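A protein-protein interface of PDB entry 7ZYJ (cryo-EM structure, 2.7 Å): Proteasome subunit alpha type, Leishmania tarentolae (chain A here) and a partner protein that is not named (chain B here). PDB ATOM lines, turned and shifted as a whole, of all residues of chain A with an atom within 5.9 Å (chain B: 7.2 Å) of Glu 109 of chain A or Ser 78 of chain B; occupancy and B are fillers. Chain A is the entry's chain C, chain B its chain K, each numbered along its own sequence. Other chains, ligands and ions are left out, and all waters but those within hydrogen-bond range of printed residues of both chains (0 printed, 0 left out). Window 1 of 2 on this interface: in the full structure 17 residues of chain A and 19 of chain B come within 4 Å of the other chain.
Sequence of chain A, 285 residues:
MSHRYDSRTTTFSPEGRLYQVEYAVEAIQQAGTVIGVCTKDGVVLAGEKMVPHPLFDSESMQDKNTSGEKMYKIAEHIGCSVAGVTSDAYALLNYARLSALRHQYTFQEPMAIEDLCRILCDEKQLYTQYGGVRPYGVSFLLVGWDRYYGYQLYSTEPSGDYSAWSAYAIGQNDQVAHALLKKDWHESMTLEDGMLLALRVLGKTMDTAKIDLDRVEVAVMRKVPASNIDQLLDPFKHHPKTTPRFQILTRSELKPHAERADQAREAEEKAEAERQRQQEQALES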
ATOM      1  N   ALA A 100     -22.145 -18.645  -6.889  1.00  0.00           N
ATOM      2  CA  ALA A 100     -20.934 -19.413  -7.152  1.00  0.00           C
ATOM      3  C   ALA A 100     -21.074 -20.854  -6.681  1.00  0.00           C
ATOM      4  O   ALA A 100     -20.684 -21.786  -7.399  1.00  0.00           O
ATOM      5  CB  ALA A 100     -19.733 -18.748  -6.481  1.00  0.00           C
ATOM      6  N   HIS A 103     -23.369 -22.759  -9.057  1.00  0.00           N
ATOM      7  CA  HIS A 103     -22.646 -23.156 -10.262  1.00  0.00           C
ATOM      8  C   HIS A 103     -21.736 -24.345  -9.986  1.00  0.00           C
ATOM      9  O   HIS A 103     -21.642 -25.266 -10.804  1.00  0.00           O
ATOM     10  CB  HIS A 103     -21.839 -21.983 -10.812  1.00  0.00           C
ATOM     11  CG  HIS A 103     -21.046 -22.324 -12.035  1.00  0.00           C
ATOM     12  ND1 HIS A 103     -21.528 -22.130 -13.312  1.00  0.00           N
ATOM     13  CD2 HIS A 103     -19.807 -22.850 -12.177  1.00  0.00           C
ATOM     14  CE1 HIS A 103     -20.618 -22.520 -14.186  1.00  0.00           C
ATOM     15  NE2 HIS A 103     -19.565 -22.962 -13.524  1.00  0.00           N
ATOM     16  N   GLN A 104     -21.049 -24.338  -8.841  1.00  0.00           N
ATOM     17  CA  GLN A 104     -20.223 -25.487  -8.480  1.00  0.00           C
ATOM     18  C   GLN A 104     -21.067 -26.740  -8.272  1.00  0.00           C
ATOM     19  O   GLN A 104     -20.627 -27.845  -8.600  1.00  0.00           O
ATOM     20  CB  GLN A 104     -19.407 -25.176  -7.226  1.00  0.00           C
ATOM     21  CG  GLN A 104     -18.727 -26.385  -6.609  1.00  0.00           C
ATOM     22  CD  GLN A 104     -17.350 -26.068  -6.069  1.00  0.00           C
ATOM     23  OE1 GLN A 104     -16.572 -25.353  -6.702  1.00  0.00           O
ATOM     24  NE2 GLN A 104     -17.038 -26.599  -4.894  1.00  0.00           N
ATOM     25  N   PHE A 107     -22.121 -27.926 -12.075  1.00  0.00           N
ATOM     26  CA  PHE A 107     -21.086 -28.326 -13.017  1.00  0.00           C
ATOM     27  C   PHE A 107     -19.855 -28.938 -12.366  1.00  0.00           C
ATOM     28  O   PHE A 107     -19.019 -29.501 -13.082  1.00  0.00           O
ATOM     29  CB  PHE A 107     -20.656 -27.124 -13.869  1.00  0.00           C
ATOM     30  CG  PHE A 107     -21.757 -26.562 -14.720  1.00  0.00           C
ATOM     31  CD1 PHE A 107     -22.032 -27.100 -15.965  1.00  0.00           C
ATOM     32  CD2 PHE A 107     -22.516 -25.495 -14.276  1.00  0.00           C
ATOM     33  CE1 PHE A 107     -23.044 -26.585 -16.747  1.00  0.00           C
ATOM     34  CE2 PHE A 107     -23.529 -24.976 -15.056  1.00  0.00           C
ATOM     35  CZ  PHE A 107     -23.793 -25.522 -16.293  1.00  0.00           C
ATOM     36  N   GLN A 108     -19.717 -28.846 -11.041  1.00  0.00           N
ATOM     37  CA  GLN A 108     -18.548 -29.355 -10.320  1.00  0.00           C
ATOM     38  C   GLN A 108     -17.251 -28.730 -10.826  1.00  0.00           C
ATOM     39  O   GLN A 108     -16.208 -29.386 -10.867  1.00  0.00           O
ATOM     40  CB  GLN A 108     -18.470 -30.884 -10.385  1.00  0.00           C
ATOM     41  CG  GLN A 108     -19.722 -31.588  -9.891  1.00  0.00           C
ATOM     42  CD  GLN A 108     -20.014 -31.304  -8.433  1.00  0.00           C
ATOM     43  OE1 GLN A 108     -19.160 -31.496  -7.569  1.00  0.00           O
ATOM     44  NE2 GLN A 108     -21.226 -30.843  -8.152  1.00  0.00           N
ATOM     45  N   GLU A 109     -17.308 -27.462 -11.213  1.00  0.00           N
ATOM     46  CA  GLU A 109     -16.139 -26.699 -11.618  1.00  0.00           C
ATOM     47  C   GLU A 109     -16.247 -25.299 -11.036  1.00  0.00           C
ATOM     48  O   GLU A 109     -17.356 -24.814 -10.783  1.00  0.00           O
ATOM     49  CB  GLU A 109     -16.009 -26.610 -13.146  1.00  0.00           C
ATOM     50  CG  GLU A 109     -17.124 -25.832 -13.818  1.00  0.00           C
ATOM     51  CD  GLU A 109     -16.998 -25.817 -15.326  1.00  0.00           C
ATOM     52  OE1 GLU A 109     -16.048 -26.435 -15.851  1.00  0.00           O
ATOM     53  OE2 GLU A 109     -17.848 -25.184 -15.988  1.00  0.00           O
ATOM     54  N   PRO A 110     -15.116 -24.633 -10.797  1.00  0.00           N
ATOM     55  CA  PRO A 110     -15.173 -23.246 -10.323  1.00  0.00           C
ATOM     56  C   PRO A 110     -15.847 -22.338 -11.338  1.00  0.00           C
ATOM     57  O   PRO A 110     -15.640 -22.462 -12.547  1.00  0.00           O
ATOM     58  CB  PRO A 110     -13.697 -22.875 -10.132  1.00  0.00           C
ATOM     59  CG  PRO A 110     -12.989 -24.178  -9.990  1.00  0.00           C
ATOM     60  CD  PRO A 110     -13.737 -25.146 -10.850  1.00  0.00           C
ATOM     61  N   MET A 111     -16.663 -21.418 -10.831  1.00  0.00           N
ATOM     62  CA  MET A 111     -17.333 -20.452 -11.688  1.00  0.00           C
ATOM     63  C   MET A 111     -16.330 -19.472 -12.278  1.00  0.00           C
ATOM     64  O   MET A 111     -15.395 -19.032 -11.602  1.00  0.00           O
ATOM     65  CB  MET A 111     -18.401 -19.695 -10.900  1.00  0.00           C
ATOM     66  CG  MET A 111     -19.584 -19.237 -11.732  1.00  0.00           C
ATOM     67  SD  MET A 111     -20.753 -18.255 -10.776  1.00  0.00           S
ATOM     68  CE  MET A 111     -22.088 -18.071 -11.955  1.00  0.00           C
ATOM     69  N   ARG A 147      -9.252 -20.766 -15.394  1.00  0.00           N
ATOM     70  CA  ARG A 147      -8.384 -21.316 -16.429  1.00  0.00           C
ATOM     71  C   ARG A 147      -8.595 -20.675 -17.794  1.00  0.00           C
ATOM     72  O   ARG A 147      -7.754 -20.862 -18.679  1.00  0.00           O
ATOM     73  CB  ARG A 147      -8.590 -22.827 -16.541  1.00  0.00           C
ATOM     74  CG  ARG A 147     -10.044 -23.255 -16.596  1.00  0.00           C
ATOM     75  CD  ARG A 147     -10.193 -24.731 -16.273  1.00  0.00           C
ATOM     76  NE  ARG A 147     -10.139 -25.560 -17.472  1.00  0.00           N
ATOM     77  CZ  ARG A 147     -11.153 -25.739 -18.306  1.00  0.00           C
ATOM     78  NH1 ARG A 147     -12.326 -25.164 -18.102  1.00  0.00           N
ATOM     79  NH2 ARG A 147     -10.986 -26.515 -19.373  1.00  0.00           N
ATOM     80  N   TYR A 148      -9.681 -19.928 -17.992  1.00  0.00           N
ATOM     81  CA  TYR A 148      -9.949 -19.360 -19.307  1.00  0.00           C
ATOM     82  C   TYR A 148      -9.182 -18.062 -19.533  1.00  0.00           C
ATOM     83  O   TYR A 148      -8.693 -17.815 -20.639  1.00  0.00           O
ATOM     84  CB  TYR A 148     -11.451 -19.127 -19.499  1.00  0.00           C
ATOM     85  CG  TYR A 148     -12.335 -20.294 -19.109  1.00  0.00           C
ATOM     86  CD1 TYR A 148     -12.610 -20.577 -17.776  1.00  0.00           C
ATOM     87  CD2 TYR A 148     -12.934 -21.087 -20.080  1.00  0.00           C
ATOM     88  CE1 TYR A 148     -13.425 -21.633 -17.423  1.00  0.00           C
ATOM     89  CE2 TYR A 148     -13.750 -22.145 -19.736  1.00  0.00           C
ATOM     90  CZ  TYR A 148     -13.994 -22.412 -18.406  1.00  0.00           C
ATOM     91  OH  TYR A 148     -14.809 -23.464 -18.058  1.00  0.00           O
ATOM     92  N   GLN B  43     -17.172 -33.239 -28.190  1.00  0.00           N
ATOM     93  CA  GLN B  43     -17.994 -33.979 -27.242  1.00  0.00           C
ATOM     94  C   GLN B  43     -19.154 -34.645 -27.962  1.00  0.00           C
ATOM     95  O   GLN B  43     -19.718 -34.080 -28.903  1.00  0.00           O
ATOM     96  CB  GLN B  43     -18.534 -33.068 -26.133  1.00  0.00           C
ATOM     97  CG  GLN B  43     -17.472 -32.512 -25.203  1.00  0.00           C
ATOM     98  CD  GLN B  43     -18.041 -31.545 -24.189  1.00  0.00           C
ATOM     99  OE1 GLN B  43     -19.191 -31.123 -24.297  1.00  0.00           O
ATOM    100  NE2 GLN B  43     -17.238 -31.189 -23.196  1.00  0.00           N
ATOM    101  N   LEU B  65     -25.870 -26.373 -23.655  1.00  0.00           N
ATOM    102  CA  LEU B  65     -24.445 -26.150 -23.887  1.00  0.00           C
ATOM    103  C   LEU B  65     -24.219 -24.993 -24.852  1.00  0.00           C
ATOM    104  O   LEU B  65     -23.334 -24.156 -24.636  1.00  0.00           O
ATOM    105  CB  LEU B  65     -23.789 -27.421 -24.420  1.00  0.00           C
ATOM    106  CG  LEU B  65     -23.693 -28.610 -23.468  1.00  0.00           C
ATOM    107  CD1 LEU B  65     -23.180 -29.826 -24.215  1.00  0.00           C
ATOM    108  CD2 LEU B  65     -22.799 -28.282 -22.285  1.00  0.00           C
ATOM    109  N   GLN B  72     -21.088 -17.166 -22.498  1.00  0.00           N
ATOM    110  CA  GLN B  72     -19.713 -17.130 -22.014  1.00  0.00           C
ATOM    111  C   GLN B  72     -18.732 -16.751 -23.116  1.00  0.00           C
ATOM    112  O   GLN B  72     -17.531 -17.009 -22.987  1.00  0.00           O
ATOM    113  CB  GLN B  72     -19.325 -18.471 -21.388  1.00  0.00           C
ATOM    114  CG  GLN B  72     -20.207 -18.883 -20.221  1.00  0.00           C
ATOM    115  CD  GLN B  72     -19.822 -20.232 -19.650  1.00  0.00           C
ATOM    116  OE1 GLN B  72     -18.866 -20.861 -20.102  1.00  0.00           O
ATOM    117  NE2 GLN B  72     -20.569 -20.685 -18.651  1.00  0.00           N
ATOM    118  N   ARG B  75     -16.741 -19.719 -24.888  1.00  0.00           N
ATOM    119  CA  ARG B  75     -15.885 -20.526 -24.024  1.00  0.00           C
ATOM    120  C   ARG B  75     -16.446 -21.941 -23.961  1.00  0.00           C
ATOM    121  O   ARG B  75     -17.550 -22.156 -23.450  1.00  0.00           O
ATOM    122  CB  ARG B  75     -15.788 -19.903 -22.635  1.00  0.00           C
ATOM    123  CG  ARG B  75     -14.923 -18.655 -22.581  1.00  0.00           C
ATOM    124  CD  ARG B  75     -14.570 -18.278 -21.154  1.00  0.00           C
ATOM    125  NE  ARG B  75     -15.564 -17.402 -20.546  1.00  0.00           N
ATOM    126  CZ  ARG B  75     -16.442 -17.787 -19.629  1.00  0.00           C
ATOM    127  NH1 ARG B  75     -16.485 -19.036 -19.195  1.00  0.00           N
ATOM    128  NH2 ARG B  75     -17.300 -16.896 -19.138  1.00  0.00           N
ATOM    129  N   HIS B  76     -15.693 -22.904 -24.481  1.00  0.00           N
ATOM    130  CA  HIS B  76     -16.151 -24.285 -24.522  1.00  0.00           C
ATOM    131  C   HIS B  76     -15.985 -24.947 -23.161  1.00  0.00           C
ATOM    132  O   HIS B  76     -14.983 -24.742 -22.470  1.00  0.00           O
ATOM    133  CB  HIS B  76     -15.387 -25.069 -25.589  1.00  0.00           C
ATOM    134  CG  HIS B  76     -15.801 -24.737 -26.989  1.00  0.00           C
ATOM    135  ND1 HIS B  76     -16.494 -25.618 -27.790  1.00  0.00           N
ATOM    136  CD2 HIS B  76     -15.624 -23.616 -27.728  1.00  0.00           C
ATOM    137  CE1 HIS B  76     -16.724 -25.057 -28.963  1.00  0.00           C
ATOM    138  NE2 HIS B  76     -16.206 -23.842 -28.952  1.00  0.00           N
ATOM    139  N   SER B  77     -16.978 -25.743 -22.780  1.00  0.00           N
ATOM    140  CA  SER B  77     -16.998 -26.393 -21.479  1.00  0.00           C
ATOM    141  C   SER B  77     -16.199 -27.688 -21.507  1.00  0.00           C
ATOM    142  O   SER B  77     -16.109 -28.367 -22.534  1.00  0.00           O
ATOM    143  CB  SER B  77     -18.437 -26.679 -21.046  1.00  0.00           C
ATOM    144  OG  SER B  77     -18.509 -26.946 -19.657  1.00  0.00           O
ATOM    145  N   SER B  78     -15.616 -28.026 -20.361  1.00  0.00           N
ATOM    146  CA  SER B  78     -14.845 -29.252 -20.239  1.00  0.00           C
ATOM    147  C   SER B  78     -15.768 -30.468 -20.219  1.00  0.00           C
ATOM    148  O   SER B  78     -16.975 -30.365 -19.982  1.00  0.00           O
ATOM    149  CB  SER B  78     -13.984 -29.221 -18.978  1.00  0.00           C
ATOM    150  OG  SER B  78     -14.779 -29.354 -17.814  1.00  0.00           O
ATOM    151  N   CYS B  79     -15.177 -31.636 -20.481  1.00  0.00           N
ATOM    152  CA  CYS B  79     -15.953 -32.872 -20.499  1.00  0.00           C
ATOM    153  C   CYS B  79     -16.553 -33.185 -19.135  1.00  0.00           C
ATOM    154  O   CYS B  79     -17.704 -33.626 -19.056  1.00  0.00           O
ATOM    155  CB  CYS B  79     -15.080 -34.035 -20.969  1.00  0.00           C
ATOM    156  SG  CYS B  79     -14.504 -33.893 -22.673  1.00  0.00           S
ATOM    157  N   GLU B  80     -15.794 -32.971 -18.058  1.00  0.00           N
ATOM    158  CA  GLU B  80     -16.314 -33.237 -16.721  1.00  0.00           C
ATOM    159  C   GLU B  80     -17.500 -32.337 -16.398  1.00  0.00           C
ATOM    160  O   GLU B  80     -18.487 -32.790 -15.808  1.00  0.00           O
ATOM    161  CB  GLU B  80     -15.208 -33.060 -15.679  1.00  0.00           C
ATOM    162  CG  GLU B  80     -14.061 -34.053 -15.796  1.00  0.00           C
ATOM    163  CD  GLU B  80     -13.105 -33.730 -16.930  1.00  0.00           C
ATOM    164  OE1 GLU B  80     -12.665 -34.670 -17.622  1.00  0.00           O
ATOM    165  OE2 GLU B  80     -12.794 -32.536 -17.129  1.00  0.00           O
ATOM    166  N   SER B  81     -17.419 -31.061 -16.775  1.00  0.00           N
ATOM    167  CA  SER B  81     -18.517 -30.134 -16.519  1.00  0.00           C
ATOM    168  C   SER B  81     -19.783 -30.563 -17.250  1.00  0.00           C
ATOM    169  O   SER B  81     -20.876 -30.579 -16.671  1.00  0.00           O
ATOM    170  CB  SER B  81     -18.102 -28.723 -16.933  1.00  0.00           C
ATOM    171  OG  SER B  81     -19.183 -27.816 -16.825  1.00  0.00           O
ATOM    172  N   THR B  82     -19.652 -30.921 -18.528  1.00  0.00           N
ATOM    173  CA  THR B  82     -20.812 -31.355 -19.302  1.00  0.00           C
ATOM    174  C   THR B  82     -21.385 -32.656 -18.753  1.00  0.00           C
ATOM    175  O   THR B  82     -22.609 -32.826 -18.679  1.00  0.00           O
ATOM    176  CB  THR B  82     -20.423 -31.516 -20.771  1.00  0.00           C
ATOM    177  OG1 THR B  82     -19.786 -30.317 -21.228  1.00  0.00           O
ATOM    178  CG2 THR B  82     -21.649 -31.772 -21.617  1.00  0.00           C
ATOM    179  N   ALA B  83     -20.511 -33.586 -18.364  1.00  0.00           N
ATOM    180  CA  ALA B  83     -20.971 -34.845 -17.792  1.00  0.00           C
ATOM    181  C   ALA B  83     -21.730 -34.612 -16.494  1.00  0.00           C
ATOM    182  O   ALA B  83     -22.776 -35.226 -16.260  1.00  0.00           O
ATOM    183  CB  ALA B  83     -19.785 -35.781 -17.558  1.00  0.00           C
ATOM    184  N   ASN B  84     -21.223 -33.719 -15.642  1.00  0.00           N
ATOM    185  CA  ASN B  84     -21.921 -33.406 -14.401  1.00  0.00           C
ATOM    186  C   ASN B  84     -23.244 -32.701 -14.664  1.00  0.00           C
ATOM    187  O   ASN B  84     -24.214 -32.924 -13.936  1.00  0.00           O
ATOM    188  CB  ASN B  84     -21.029 -32.557 -13.502  1.00  0.00           C
ATOM    189  CG  ASN B  84     -19.968 -33.376 -12.804  1.00  0.00           C
ATOM    190  OD1 ASN B  84     -20.274 -34.215 -11.958  1.00  0.00           O
ATOM    191  ND2 ASN B  84     -18.711 -33.143 -13.159  1.00  0.00           N
ATOM    192  N   PHE B 107     -20.912 -40.979 -22.521  1.00  0.00           N
ATOM    193  CA  PHE B 107     -20.478 -39.641 -22.900  1.00  0.00           C
ATOM    194  C   PHE B 107     -18.983 -39.661 -23.184  1.00  0.00           C
ATOM    195  O   PHE B 107     -18.185 -40.000 -22.305  1.00  0.00           O
ATOM    196  CB  PHE B 107     -20.805 -38.630 -21.800  1.00  0.00           C
ATOM    197  CG  PHE B 107     -20.149 -37.295 -21.993  1.00  0.00           C
ATOM    198  CD1 PHE B 107     -20.526 -36.467 -23.034  1.00  0.00           C
ATOM    199  CD2 PHE B 107     -19.157 -36.866 -21.131  1.00  0.00           C
ATOM    200  CE1 PHE B 107     -19.926 -35.239 -23.214  1.00  0.00           C
ATOM    201  CE2 PHE B 107     -18.553 -35.639 -21.307  1.00  0.00           C
ATOM    202  CZ  PHE B 107     -18.938 -34.824 -22.349  1.00  0.00           C
ATOM    203  N   TYR B 110     -12.994 -35.104 -25.800  1.00  0.00           N
ATOM    204  CA  TYR B 110     -11.563 -34.829 -25.786  1.00  0.00           C
ATOM    205  C   TYR B 110     -11.358 -33.430 -25.230  1.00  0.00           C
ATOM    206  O   TYR B 110     -11.941 -32.467 -25.739  1.00  0.00           O
ATOM    207  CB  TYR B 110     -10.960 -34.955 -27.186  1.00  0.00           C
ATOM    208  CG  TYR B 110      -9.465 -35.174 -27.189  1.00  0.00           C
ATOM    209  CD1 TYR B 110      -8.588 -34.110 -27.033  1.00  0.00           C
ATOM    210  CD2 TYR B 110      -8.931 -36.445 -27.347  1.00  0.00           C
ATOM    211  CE1 TYR B 110      -7.222 -34.307 -27.035  1.00  0.00           C
ATOM    212  CE2 TYR B 110      -7.568 -36.651 -27.350  1.00  0.00           C
ATOM    213  CZ  TYR B 110      -6.718 -35.579 -27.193  1.00  0.00           C
ATOM    214  OH  TYR B 110      -5.357 -35.778 -27.195  1.00  0.00           O
ATOM    215  N   ASP B 111     -10.535 -33.318 -24.192  1.00  0.00           N
ATOM    216  CA  ASP B 111     -10.283 -32.042 -23.538  1.00  0.00           C
ATOM    217  C   ASP B 111      -9.027 -31.409 -24.121  1.00  0.00           C
ATOM    218  O   ASP B 111      -7.975 -32.052 -24.191  1.00  0.00           O
ATOM    219  CB  ASP B 111     -10.140 -32.224 -22.028  1.00  0.00           C
ATOM    220  CG  ASP B 111     -11.476 -32.265 -21.318  1.00  0.00           C
ATOM    221  OD1 ASP B 111     -12.435 -31.643 -21.821  1.00  0.00           O
ATOM    222  OD2 ASP B 111     -11.569 -32.916 -20.256  1.00  0.00           O
ATOM    223  N   THR B 112      -9.140 -30.158 -24.538  1.00  0.00           N
ATOM    224  CA  THR B 112      -8.017 -29.391 -25.043  1.00  0.00           C
ATOM    225  C   THR B 112      -7.851 -28.113 -24.226  1.00  0.00           C
ATOM    226  O   THR B 112      -8.830 -27.583 -23.693  1.00  0.00           O
ATOM    227  CB  THR B 112      -8.208 -29.025 -26.520  1.00  0.00           C
ATOM    228  OG1 THR B 112      -9.383 -28.219 -26.668  1.00  0.00           O
ATOM    229  CG2 THR B 112      -8.350 -30.278 -27.366  1.00  0.00           C
ATOM    230  N   VAL B 114      -8.120 -24.630 -23.250  1.00  0.00           N
ATOM    231  CA  VAL B 114      -8.913 -23.526 -23.781  1.00  0.00           C
ATOM    232  C   VAL B 114      -8.063 -22.272 -23.935  1.00  0.00           C
ATOM    233  O   VAL B 114      -8.314 -21.450 -24.824  1.00  0.00           O
ATOM    234  CB  VAL B 114     -10.145 -23.272 -22.892  1.00  0.00           C
ATOM    235  CG1 VAL B 114     -11.063 -24.482 -22.906  1.00  0.00           C
ATOM    236  CG2 VAL B 114      -9.725 -22.937 -21.470  1.00  0.00           C
ATOM    237  N   ASP B 118      -4.780 -22.466 -19.003  1.00  0.00           N
ATOM    238  CA  ASP B 118      -5.433 -23.722 -18.662  1.00  0.00           C
ATOM    239  C   ASP B 118      -4.417 -24.750 -18.179  1.00  0.00           C
ATOM    240  O   ASP B 118      -3.318 -24.871 -18.728  1.00  0.00           O
ATOM    241  CB  ASP B 118      -6.192 -24.266 -19.871  1.00  0.00           C
ATOM    242  CG  ASP B 118      -7.264 -25.268 -19.486  1.00  0.00           C
ATOM    243  OD1 ASP B 118      -7.244 -25.757 -18.337  1.00  0.00           O
ATOM    244  OD2 ASP B 118      -8.124 -25.572 -20.337  1.00  0.00           O
ATOM    245  N   VAL B 121      -7.491 -31.146 -17.750  1.00  0.00           N
ATOM    246  CA  VAL B 121      -7.363 -32.417 -18.452  1.00  0.00           C
ATOM    247  C   VAL B 121      -6.984 -32.165 -19.905  1.00  0.00           C
ATOM    248  O   VAL B 121      -7.457 -31.217 -20.541  1.00  0.00           O
ATOM    249  CB  VAL B 121      -8.677 -33.218 -18.336  1.00  0.00           C
ATOM    250  CG1 VAL B 121      -8.689 -34.404 -19.291  1.00  0.00           C
ATOM    251  CG2 VAL B 121      -8.893 -33.678 -16.906  1.00  0.00           C
ATOM    252  N   GLN B 125     -11.704 -38.448 -22.535  1.00  0.00           N
ATOM    253  CA  GLN B 125     -12.573 -38.685 -21.392  1.00  0.00           C
ATOM    254  C   GLN B 125     -13.767 -39.529 -21.814  1.00  0.00           C
ATOM    255  O   GLN B 125     -14.362 -39.295 -22.872  1.00  0.00           O
ATOM    256  CB  GLN B 125     -13.066 -37.362 -20.790  1.00  0.00           C
ATOM    257  CG  GLN B 125     -11.971 -36.477 -20.219  1.00  0.00           C
ATOM    258  CD  GLN B 125     -11.264 -37.107 -19.038  1.00  0.00           C
ATOM    259  OE1 GLN B 125     -10.103 -37.502 -19.132  1.00  0.00           O
ATOM    260  NE2 GLN B 125     -11.965 -37.207 -17.916  1.00  0.00           N
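Glu 109 of chain A touches just these residues of chain B: Ser 78 and Ser 81. Ser 78 of chain B touches just one residue of chain A: Glu 109. Of the printed residues of chain B, Gln 108 of chain A touches Asn 84 (3.4 Å). Of the printed residues of chain A, Val 114 of chain B touches Arg 147 and Tyr 148. Of the printed residues of chain B, Arg 147 of chain A touches Val 114 and Asp 118. Of the printed residues of chain A, Arg 75 of chain B touches Tyr 148. The nearest residue of chain B that does not touch Glu 109 of chain A is Ser 77 of chain B (4.1 Å). The nearest printed residue of chain A that does not touch Asn 84 of chain B is Glu 109 of chain A (6.2 Å).
Hydrophobic or aromatic side chains of chain B within 4 Å of the printed part of chain A: Val 114. Among the printed residues, 10 pairs touch across the chains. Among the printed residues, Asp or Glu carboxylates within 4 Å of a Lys or Arg side-chain nitrogen of the other chain: Arg 147 of chain A with Asp 118 of chain B.
Phe 107 of chain A touches Ser 81 of chain B (CD1 to OG, 3.1 Å). Phe 107 of chain A touches Asn 84 of chain B (O to ND2, 3.7 Å). Asn 84 of chain B touches Gln 108 of chain A (OD1 to CG, 3.4 Å). Glu 109 of chain A touches Ser 78 of chain B (OE1 to OG, 3.7 Å). O of Arg 147 of chain A touches CG2 of Val 114 of chain B, 3.998 Å away. Tyr 148 of chain A touches Arg 75 of chain B (CD2 to CD, 3.4 Å). His 76 of chain B touches Tyr 148 of chain A (O to CE2, 3.97 Å). Tyr 148 of chain A touches Val 114 of chain B (CD2 to CG2, 3.96 Å).
The backbone carbonyl oxygen (O) of Ser 78 of chain B sits at hydrogen-bond distance from the side-chain amide nitrogen (NE2) of Gln 43 of chain B (3.3 Å). The side-chain hydroxyl (OG) of Ser 78 of chain B lies within hydrogen-bond range of the backbone NH (N) of Ser 81 of chain B (3.3 Å). The guanidinium group (NH1) of Arg 147 of chain A is in hydrogen-bond range of the side-chain hydroxyl (OH) of Tyr 148 of chain A, at 3.0 Å. The side-chain hydroxyl (OG) of Ser 77 of chain B sits at hydrogen-bond distance from the side-chain hydroxyl (OG) of Ser 81 of chain B (3.0 Å). N of Val 114 of chain B sits at hydrogen-bond distance from OD2 of Asp 118 of chain B (3.1 Å). The side-chain amide oxygen (OE1) of Gln 72 of chain B sits at hydrogen-bond distance from the guanidinium group (NH1) of Arg 75 of chain B, 3.1 Å away.
The guanidinium group of Arg 147 of chain A lies within salt-bridge range of the side-chain carboxylate of Asp 118 of chain B (3.0 Å). The side-chain carboxylate of Glu 109 of chain A lies within hydrogen-bond range of the side-chain hydroxyl of Ser 81 of chain B, 3.1 Å away.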
